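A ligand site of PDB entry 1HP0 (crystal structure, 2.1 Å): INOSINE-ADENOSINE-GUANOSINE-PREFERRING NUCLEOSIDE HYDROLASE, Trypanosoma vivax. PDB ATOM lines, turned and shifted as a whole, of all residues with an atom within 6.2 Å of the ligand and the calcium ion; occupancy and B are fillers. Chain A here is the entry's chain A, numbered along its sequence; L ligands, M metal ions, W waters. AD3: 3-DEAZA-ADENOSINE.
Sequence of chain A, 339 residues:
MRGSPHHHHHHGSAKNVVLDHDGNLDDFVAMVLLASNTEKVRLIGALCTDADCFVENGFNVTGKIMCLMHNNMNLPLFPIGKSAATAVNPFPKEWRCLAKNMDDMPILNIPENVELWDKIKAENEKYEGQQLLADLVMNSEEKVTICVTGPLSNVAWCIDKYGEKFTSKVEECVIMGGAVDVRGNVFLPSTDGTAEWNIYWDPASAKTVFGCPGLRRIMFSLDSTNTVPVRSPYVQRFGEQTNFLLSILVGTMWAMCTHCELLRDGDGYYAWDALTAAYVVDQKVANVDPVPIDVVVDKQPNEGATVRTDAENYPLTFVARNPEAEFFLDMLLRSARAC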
ATOM      1  N   HIS A  21       7.550  31.272  19.147  1.00  0.00           N
ATOM      2  CA  HIS A  21       7.012  29.943  18.846  1.00  0.00           C
ATOM      3  C   HIS A  21       7.459  28.816  19.756  1.00  0.00           C
ATOM      4  O   HIS A  21       8.345  28.991  20.588  1.00  0.00           O
ATOM      5  CB  HIS A  21       7.380  29.586  17.401  1.00  0.00           C
ATOM      6  CG  HIS A  21       8.808  29.174  17.224  1.00  0.00           C
ATOM      7  ND1 HIS A  21       9.227  27.875  17.366  1.00  0.00           N
ATOM      8  CD2 HIS A  21       9.928  29.905  16.960  1.00  0.00           C
ATOM      9  CE1 HIS A  21      10.539  27.806  17.188  1.00  0.00           C
ATOM     10  NE2 HIS A  21      10.987  29.022  16.947  1.00  0.00           N
ATOM     11  N   ASP A  22       6.835  27.648  19.589  1.00  0.00           N
ATOM     12  CA  ASP A  22       7.234  26.505  20.396  1.00  0.00           C
ATOM     13  C   ASP A  22       7.750  25.322  19.568  1.00  0.00           C
ATOM     14  O   ASP A  22       7.626  24.157  19.947  1.00  0.00           O
ATOM     15  CB  ASP A  22       6.104  26.065  21.345  1.00  0.00           C
ATOM     16  CG  ASP A  22       4.876  25.606  20.615  1.00  0.00           C
ATOM     17  OD1 ASP A  22       4.022  24.989  21.272  1.00  0.00           O
ATOM     18  OD2 ASP A  22       4.775  25.863  19.409  1.00  0.00           O
ATOM     19  N   GLY A  23       8.307  25.642  18.406  1.00  0.00           N
ATOM     20  CA  GLY A  23       8.928  24.639  17.567  1.00  0.00           C
ATOM     21  C   GLY A  23       8.275  23.376  17.039  1.00  0.00           C
ATOM     22  O   GLY A  23       8.942  22.335  16.944  1.00  0.00           O
ATOM     23  N   ASN A  24       6.992  23.402  16.698  1.00  0.00           N
ATOM     24  CA  ASN A  24       6.440  22.215  16.103  1.00  0.00           C
ATOM     25  C   ASN A  24       6.523  22.453  14.596  1.00  0.00           C
ATOM     26  O   ASN A  24       7.113  23.438  14.162  1.00  0.00           O
ATOM     27  CB  ASN A  24       5.016  21.950  16.520  1.00  0.00           C
ATOM     28  CG  ASN A  24       4.749  20.478  16.596  1.00  0.00           C
ATOM     29  OD1 ASN A  24       4.973  19.857  17.642  1.00  0.00           O
ATOM     30  ND2 ASN A  24       4.337  19.880  15.467  1.00  0.00           N
ATOM     31  N   LEU A  25       5.977  21.540  13.787  1.00  0.00           N
ATOM     32  CA  LEU A  25       6.080  21.693  12.330  1.00  0.00           C
ATOM     33  C   LEU A  25       5.458  22.966  11.783  1.00  0.00           C
ATOM     34  O   LEU A  25       6.081  23.678  11.015  1.00  0.00           O
ATOM     35  CB  LEU A  25       5.493  20.472  11.613  1.00  0.00           C
ATOM     36  CG  LEU A  25       6.271  19.140  11.644  1.00  0.00           C
ATOM     37  CD1 LEU A  25       7.720  19.316  11.196  1.00  0.00           C
ATOM     38  CD2 LEU A  25       6.254  18.595  13.032  1.00  0.00           C
ATOM     39  N   ASP A  26       4.224  23.267  12.182  1.00  0.00           N
ATOM     40  CA  ASP A  26       3.600  24.478  11.675  1.00  0.00           C
ATOM     41  C   ASP A  26       4.283  25.761  12.175  1.00  0.00           C
ATOM     42  O   ASP A  26       4.183  26.797  11.531  1.00  0.00           O
ATOM     43  CB  ASP A  26       2.082  24.468  11.977  1.00  0.00           C
ATOM     44  CG  ASP A  26       1.769  24.430  13.460  1.00  0.00           C
ATOM     45  OD1 ASP A  26       2.465  23.719  14.212  1.00  0.00           O
ATOM     46  OD2 ASP A  26       0.795  25.089  13.860  1.00  0.00           O
ATOM     47  N   ASP A  27       4.994  25.689  13.303  1.00  0.00           N
ATOM     48  CA  ASP A  27       5.724  26.851  13.814  1.00  0.00           C
ATOM     49  C   ASP A  27       6.830  27.181  12.813  1.00  0.00           C
ATOM     50  O   ASP A  27       7.088  28.331  12.528  1.00  0.00           O
ATOM     51  CB  ASP A  27       6.387  26.533  15.168  1.00  0.00           C
ATOM     52  CG  ASP A  27       5.389  26.350  16.275  1.00  0.00           C
ATOM     53  OD1 ASP A  27       5.068  27.338  16.958  1.00  0.00           O
ATOM     54  OD2 ASP A  27       4.917  25.215  16.436  1.00  0.00           O
ATOM     55  N   ASP A  52       5.542  22.745  22.772  1.00  0.00           N
ATOM     56  CA  ASP A  52       5.270  21.650  21.856  1.00  0.00           C
ATOM     57  C   ASP A  52       6.556  21.162  21.169  1.00  0.00           C
ATOM     58  O   ASP A  52       6.528  20.688  20.015  1.00  0.00           O
ATOM     59  CB  ASP A  52       4.252  22.061  20.797  1.00  0.00           C
ATOM     60  CG  ASP A  52       3.542  20.875  20.175  1.00  0.00           C
ATOM     61  OD1 ASP A  52       2.785  21.072  19.209  1.00  0.00           O
ATOM     62  OD2 ASP A  52       3.723  19.740  20.667  1.00  0.00           O
ATOM     63  N   PHE A  91       2.353  19.546  26.642  1.00  0.00           N
ATOM     64  CA  PHE A  91       1.900  18.912  25.401  1.00  0.00           C
ATOM     65  C   PHE A  91       2.244  17.416  25.461  1.00  0.00           C
ATOM     66  O   PHE A  91       3.172  17.006  26.186  1.00  0.00           O
ATOM     67  CB  PHE A  91       2.635  19.511  24.183  1.00  0.00           C
ATOM     68  CG  PHE A  91       2.063  20.817  23.675  1.00  0.00           C
ATOM     69  CD1 PHE A  91       2.369  22.028  24.273  1.00  0.00           C
ATOM     70  CD2 PHE A  91       1.208  20.813  22.559  1.00  0.00           C
ATOM     71  CE1 PHE A  91       1.839  23.234  23.793  1.00  0.00           C
ATOM     72  CE2 PHE A  91       0.679  22.008  22.060  1.00  0.00           C
ATOM     73  CZ  PHE A  91       0.988  23.221  22.677  1.00  0.00           C
ATOM     74  N   TRP A  95       4.092  14.541  20.291  1.00  0.00           N
ATOM     75  CA  TRP A  95       4.179  15.633  19.335  1.00  0.00           C
ATOM     76  C   TRP A  95       5.426  16.491  19.494  1.00  0.00           C
ATOM     77  O   TRP A  95       5.944  17.016  18.513  1.00  0.00           O
ATOM     78  CB  TRP A  95       2.976  16.576  19.444  1.00  0.00           C
ATOM     79  CG  TRP A  95       1.636  15.930  19.422  1.00  0.00           C
ATOM     80  CD1 TRP A  95       1.325  14.686  18.952  1.00  0.00           C
ATOM     81  CD2 TRP A  95       0.414  16.518  19.860  1.00  0.00           C
ATOM     82  NE1 TRP A  95      -0.023  14.468  19.074  1.00  0.00           N
ATOM     83  CE2 TRP A  95      -0.611  15.578  19.628  1.00  0.00           C
ATOM     84  CE3 TRP A  95       0.084  17.761  20.427  1.00  0.00           C
ATOM     85  CZ2 TRP A  95      -1.956  15.839  19.937  1.00  0.00           C
ATOM     86  CZ3 TRP A  95      -1.252  18.026  20.734  1.00  0.00           C
ATOM     87  CH2 TRP A  95      -2.251  17.061  20.481  1.00  0.00           C
ATOM     88  N   THR A 149       2.978  31.774  18.051  1.00  0.00           N
ATOM     89  CA  THR A 149       2.475  30.487  17.575  1.00  0.00           C
ATOM     90  C   THR A 149       2.591  29.383  18.604  1.00  0.00           C
ATOM     91  O   THR A 149       2.283  28.209  18.328  1.00  0.00           O
ATOM     92  CB  THR A 149       3.175  30.057  16.295  1.00  0.00           C
ATOM     93  OG1 THR A 149       4.581  29.909  16.543  1.00  0.00           O
ATOM     94  CG2 THR A 149       2.964  31.087  15.199  1.00  0.00           C
ATOM     95  N   GLY A 150       3.056  29.748  19.789  1.00  0.00           N
ATOM     96  CA  GLY A 150       3.173  28.800  20.887  1.00  0.00           C
ATOM     97  C   GLY A 150       2.346  29.405  22.019  1.00  0.00           C
ATOM     98  O   GLY A 150       1.512  30.287  21.753  1.00  0.00           O
ATOM     99  N   PRO A 151       2.524  28.968  23.280  1.00  0.00           N
ATOM    100  CA  PRO A 151       1.748  29.517  24.401  1.00  0.00           C
ATOM    101  C   PRO A 151       2.031  30.992  24.669  1.00  0.00           C
ATOM    102  O   PRO A 151       3.024  31.550  24.214  1.00  0.00           O
ATOM    103  CB  PRO A 151       2.145  28.619  25.583  1.00  0.00           C
ATOM    104  CG  PRO A 151       2.461  27.297  24.907  1.00  0.00           C
ATOM    105  CD  PRO A 151       3.249  27.743  23.672  1.00  0.00           C
ATOM    106  N   MET A 176      -1.925  32.617  17.651  1.00  0.00           N
ATOM    107  CA  MET A 176      -2.587  31.381  17.233  1.00  0.00           C
ATOM    108  C   MET A 176      -2.992  30.735  18.551  1.00  0.00           C
ATOM    109  O   MET A 176      -2.139  30.415  19.397  1.00  0.00           O
ATOM    110  CB  MET A 176      -1.648  30.443  16.479  1.00  0.00           C
ATOM    111  CG  MET A 176      -2.355  29.187  15.907  1.00  0.00           C
ATOM    112  SD  MET A 176      -2.855  27.974  17.177  1.00  0.00           S
ATOM    113  CE  MET A 176      -4.606  27.726  16.864  1.00  0.00           C
ATOM    114  N   ASN A 185      -9.336  21.405  20.953  1.00  0.00           N
ATOM    115  CA  ASN A 185      -8.605  20.238  20.468  1.00  0.00           C
ATOM    116  C   ASN A 185      -7.791  19.580  21.573  1.00  0.00           C
ATOM    117  O   ASN A 185      -6.907  18.769  21.310  1.00  0.00           O
ATOM    118  CB  ASN A 185      -7.712  20.565  19.265  1.00  0.00           C
ATOM    119  CG  ASN A 185      -6.647  21.633  19.554  1.00  0.00           C
ATOM    120  OD1 ASN A 185      -6.466  22.068  20.690  1.00  0.00           O
ATOM    121  ND2 ASN A 185      -5.934  22.033  18.501  1.00  0.00           N
ATOM    122  N   GLU A 196      -8.186  24.770  23.619  1.00  0.00           N
ATOM    123  CA  GLU A 196      -7.200  24.597  22.555  1.00  0.00           C
ATOM    124  C   GLU A 196      -5.833  24.517  23.268  1.00  0.00           C
ATOM    125  O   GLU A 196      -5.638  25.173  24.289  1.00  0.00           O
ATOM    126  CB  GLU A 196      -7.270  25.777  21.570  1.00  0.00           C
ATOM    127  CG  GLU A 196      -6.222  25.744  20.476  1.00  0.00           C
ATOM    128  CD  GLU A 196      -4.879  26.299  20.939  1.00  0.00           C
ATOM    129  OE1 GLU A 196      -3.829  25.823  20.440  1.00  0.00           O
ATOM    130  OE2 GLU A 196      -4.887  27.207  21.792  1.00  0.00           O
ATOM    131  N   TRP A 197      -4.916  23.727  22.722  1.00  0.00           N
ATOM    132  CA  TRP A 197      -3.598  23.511  23.319  1.00  0.00           C
ATOM    133  C   TRP A 197      -2.704  24.667  23.775  1.00  0.00           C
ATOM    134  O   TRP A 197      -2.228  24.624  24.914  1.00  0.00           O
ATOM    135  CB  TRP A 197      -2.763  22.554  22.441  1.00  0.00           C
ATOM    136  CG  TRP A 197      -3.113  21.142  22.706  1.00  0.00           C
ATOM    137  CD1 TRP A 197      -3.934  20.345  21.973  1.00  0.00           C
ATOM    138  CD2 TRP A 197      -2.729  20.376  23.850  1.00  0.00           C
ATOM    139  NE1 TRP A 197      -4.091  19.133  22.588  1.00  0.00           N
ATOM    140  CE2 TRP A 197      -3.363  19.124  23.746  1.00  0.00           C
ATOM    141  CE3 TRP A 197      -1.922  20.630  24.968  1.00  0.00           C
ATOM    142  CZ2 TRP A 197      -3.222  18.120  24.706  1.00  0.00           C
ATOM    143  CZ3 TRP A 197      -1.768  19.620  25.926  1.00  0.00           C
ATOM    144  CH2 TRP A 197      -2.419  18.390  25.782  1.00  0.00           C
ATOM    145  N   ASN A 198      -2.440  25.664  22.929  1.00  0.00           N
ATOM    146  CA  ASN A 198      -1.582  26.762  23.368  1.00  0.00           C
ATOM    147  C   ASN A 198      -2.093  27.488  24.618  1.00  0.00           C
ATOM    148  O   ASN A 198      -1.306  27.864  25.487  1.00  0.00           O
ATOM    149  CB  ASN A 198      -1.365  27.793  22.248  1.00  0.00           C
ATOM    150  CG  ASN A 198      -0.564  27.240  21.082  1.00  0.00           C
ATOM    151  OD1 ASN A 198       0.182  26.260  21.222  1.00  0.00           O
ATOM    152  ND2 ASN A 198      -0.706  27.873  19.931  1.00  0.00           N
ATOM    153  N   LEU A 222      -9.270  28.123  16.727  1.00  0.00           N
ATOM    154  CA  LEU A 222      -9.659  27.019  15.860  1.00  0.00           C
ATOM    155  C   LEU A 222     -10.797  27.392  14.886  1.00  0.00           C
ATOM    156  O   LEU A 222     -10.997  26.723  13.868  1.00  0.00           O
ATOM    157  CB  LEU A 222      -9.999  25.777  16.692  1.00  0.00           C
ATOM    158  CG  LEU A 222      -8.869  25.312  17.619  1.00  0.00           C
ATOM    159  CD1 LEU A 222      -9.223  23.954  18.172  1.00  0.00           C
ATOM    160  CD2 LEU A 222      -7.501  25.248  16.869  1.00  0.00           C
ATOM    161  N   GLY A 268      -7.114  16.148  10.827  1.00  0.00           N
ATOM    162  CA  GLY A 268      -6.313  15.725  11.971  1.00  0.00           C
ATOM    163  C   GLY A 268      -5.140  16.661  12.232  1.00  0.00           C
ATOM    164  O   GLY A 268      -4.672  16.786  13.369  1.00  0.00           O
ATOM    165  N   TYR A 269      -4.674  17.308  11.160  1.00  0.00           N
ATOM    166  CA  TYR A 269      -3.553  18.250  11.224  1.00  0.00           C
ATOM    167  C   TYR A 269      -3.882  19.515  10.399  1.00  0.00           C
ATOM    168  O   TYR A 269      -4.224  19.434   9.216  1.00  0.00           O
ATOM    169  CB  TYR A 269      -2.285  17.595  10.677  1.00  0.00           C
ATOM    170  CG  TYR A 269      -1.391  16.986  11.731  1.00  0.00           C
ATOM    171  CD1 TYR A 269      -1.822  15.895  12.494  1.00  0.00           C
ATOM    172  CD2 TYR A 269      -0.121  17.506  11.986  1.00  0.00           C
ATOM    173  CE1 TYR A 269      -1.003  15.338  13.491  1.00  0.00           C
ATOM    174  CE2 TYR A 269       0.707  16.951  12.972  1.00  0.00           C
ATOM    175  CZ  TYR A 269       0.258  15.875  13.724  1.00  0.00           C
ATOM    176  OH  TYR A 269       1.071  15.337  14.720  1.00  0.00           O
ATOM    177  N   TRP A 272      -2.266  25.517  11.372  1.00  0.00           N
ATOM    178  CA  TRP A 272      -2.515  26.489  12.435  1.00  0.00           C
ATOM    179  C   TRP A 272      -1.602  27.702  12.451  1.00  0.00           C
ATOM    180  O   TRP A 272      -2.039  28.821  12.163  1.00  0.00           O
ATOM    181  CB  TRP A 272      -2.439  25.808  13.818  1.00  0.00           C
ATOM    182  CG  TRP A 272      -3.262  24.551  14.009  1.00  0.00           C
ATOM    183  CD1 TRP A 272      -4.584  24.457  14.325  1.00  0.00           C
ATOM    184  CD2 TRP A 272      -2.757  23.197  13.993  1.00  0.00           C
ATOM    185  NE1 TRP A 272      -4.941  23.142  14.515  1.00  0.00           N
ATOM    186  CE2 TRP A 272      -3.841  22.345  14.320  1.00  0.00           C
ATOM    187  CE3 TRP A 272      -1.505  22.637  13.751  1.00  0.00           C
ATOM    188  CZ2 TRP A 272      -3.699  20.946  14.416  1.00  0.00           C
ATOM    189  CZ3 TRP A 272      -1.358  21.229  13.848  1.00  0.00           C
ATOM    190  CH2 TRP A 272      -2.456  20.416  14.181  1.00  0.00           C
ATOM    191  N   ASP A 273      -0.335  27.488  12.800  1.00  0.00           N
ATOM    192  CA  ASP A 273       0.630  28.576  12.897  1.00  0.00           C
ATOM    193  C   ASP A 273       0.956  29.255  11.567  1.00  0.00           C
ATOM    194  O   ASP A 273       1.201  30.453  11.522  1.00  0.00           O
ATOM    195  CB  ASP A 273       1.942  28.070  13.527  1.00  0.00           C
ATOM    196  CG  ASP A 273       1.730  27.505  14.927  1.00  0.00           C
ATOM    197  OD1 ASP A 273       0.709  27.833  15.566  1.00  0.00           O
ATOM    198  OD2 ASP A 273       2.586  26.723  15.379  1.00  0.00           O
HETATM  199  O5' AD3 L   1      -3.479  23.974  18.721  1.00  0.00           O
HETATM  200  C5' AD3 L   1      -2.475  24.480  17.853  1.00  0.00           C
HETATM  201  C4' AD3 L   1      -1.091  24.694  18.533  1.00  0.00           C
HETATM  202  O4' AD3 L   1      -0.806  23.293  18.843  1.00  0.00           O
HETATM  203  C3' AD3 L   1      -0.341  25.066  17.243  1.00  0.00           C
HETATM  204  O3' AD3 L   1       0.377  26.260  17.546  1.00  0.00           O
HETATM  205  C2' AD3 L   1       0.510  23.815  16.874  1.00  0.00           C
HETATM  206  O2' AD3 L   1       1.921  23.969  16.730  1.00  0.00           O
HETATM  207  C1' AD3 L   1       0.209  22.793  17.974  1.00  0.00           C
HETATM  208  N9  AD3 L   1       0.094  21.350  17.574  1.00  0.00           N
HETATM  209  C8  AD3 L   1       1.091  20.563  16.953  1.00  0.00           C
HETATM  210  N7  AD3 L   1       0.744  19.321  16.683  1.00  0.00           N
HETATM  211  C5  AD3 L   1      -0.581  19.259  17.147  1.00  0.00           C
HETATM  212  C6  AD3 L   1      -1.574  18.191  17.164  1.00  0.00           C
HETATM  213  N6  AD3 L   1      -1.356  16.977  16.681  1.00  0.00           N
HETATM  214  N1  AD3 L   1      -2.816  18.480  17.709  1.00  0.00           N
HETATM  215  C2  AD3 L   1      -3.074  19.723  18.204  1.00  0.00           C
HETATM  216  C3  AD3 L   1      -2.252  20.796  18.263  1.00  0.00           C
HETATM  217  C4  AD3 L   1      -1.000  20.499  17.698  1.00  0.00           C
HETATM  218 CA    CA M   1       2.940  26.090  17.734  1.00  0.00          CA
HETATM  219  O   HOH W   1       2.031  24.907  19.817  1.00  0.00           O
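The side-chain carboxylate (OD1) of Asp 26 sits close to an oxygen (O2') of the ligand.
The side-chain amide nitrogen (ND2) of Asn 185 sits at hydrogen-bond distance from an oxygen (O5') of the ligand (3.1 Å).
The side-chain carboxylate of Glu 196 lies within hydrogen-bond range of an oxygen (O5') of the ligand, at 2.5 Å.
An oxygen (O3') of the ligand lies close to the side-chain amide nitrogen (ND2) of Asn 198.
The side-chain sulfur of Met 176 lies close to an oxygen (O3') of the ligand (3.7 Å).
The side-chain carboxylate (OD1) of Asp 52 sits close to a nitrogen (N9) of the ligand (3.2 Å).
Merely in contact with the ligand: Trp 95, Tyr 269, Asn 24, Trp 272, Phe 91 and Trp 197.
Hydrophobic or aromatic side chains that line the ligand: Phe 91, Trp 95, Met 176, Trp 197, Tyr 269 and Trp 272.
The calcium ion is bound by the backbone carbonyl oxygen (O) of Thr 149 (2.3 Å), the side-chain carboxylate (OD2) of Asp 273 (2.5 Å), the side-chain carboxylate (OD2) of Asp 22 (2.5 Å), the side-chain carboxylate (OD2) of Asp 27 (2.5 Å), an oxygen (O2') of the ligand (2.6 Å), water W1 (2.6 Å), an oxygen (O3') of the ligand (2.6 Å) and the side-chain carboxylate (OD1) of Asp 27 (2.6 Å).
The calcium ion has eight donor atoms within binding distance.
OD2 of Asp 27 sits close to N of Asn 24.
The backbone NH (N) of Trp 197 is in hydrogen-bond range of the side-chain amide oxygen (OD1) of Asn 185 (3.0 Å).
The side-chain carboxylate (OE1) of Glu 196 lies within hydrogen-bond range of the backbone NH (N) of Asn 198, at 2.9 Å.
The backbone carbonyl oxygen (O) of Thr 149 lies close to the side-chain amide nitrogen (ND2) of Asn 198, 3.4 Å away.
The backbone NH (N) of Asp 273 sits close to the side-chain carboxylate (OD2) of Asp 26, at 2.9 Å.
The backbone NH (N) of Asp 52 sits close to the side-chain carboxylate (OD1) of Asp 22.
ND2 of Asn 198 sits at hydrogen-bond distance from O of Met 176 (3.0 Å).
The side-chain amide oxygen (OD1) of Asn 24 lies close to the backbone carbonyl oxygen (O) of Trp 95.
Within 4 Å of the calcium ion: Asp 22, Asp 27, Thr 149 and Asp 273.
The nearest printed residue that does not touch the calcium ion is Gly 150 (4.2 Å).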
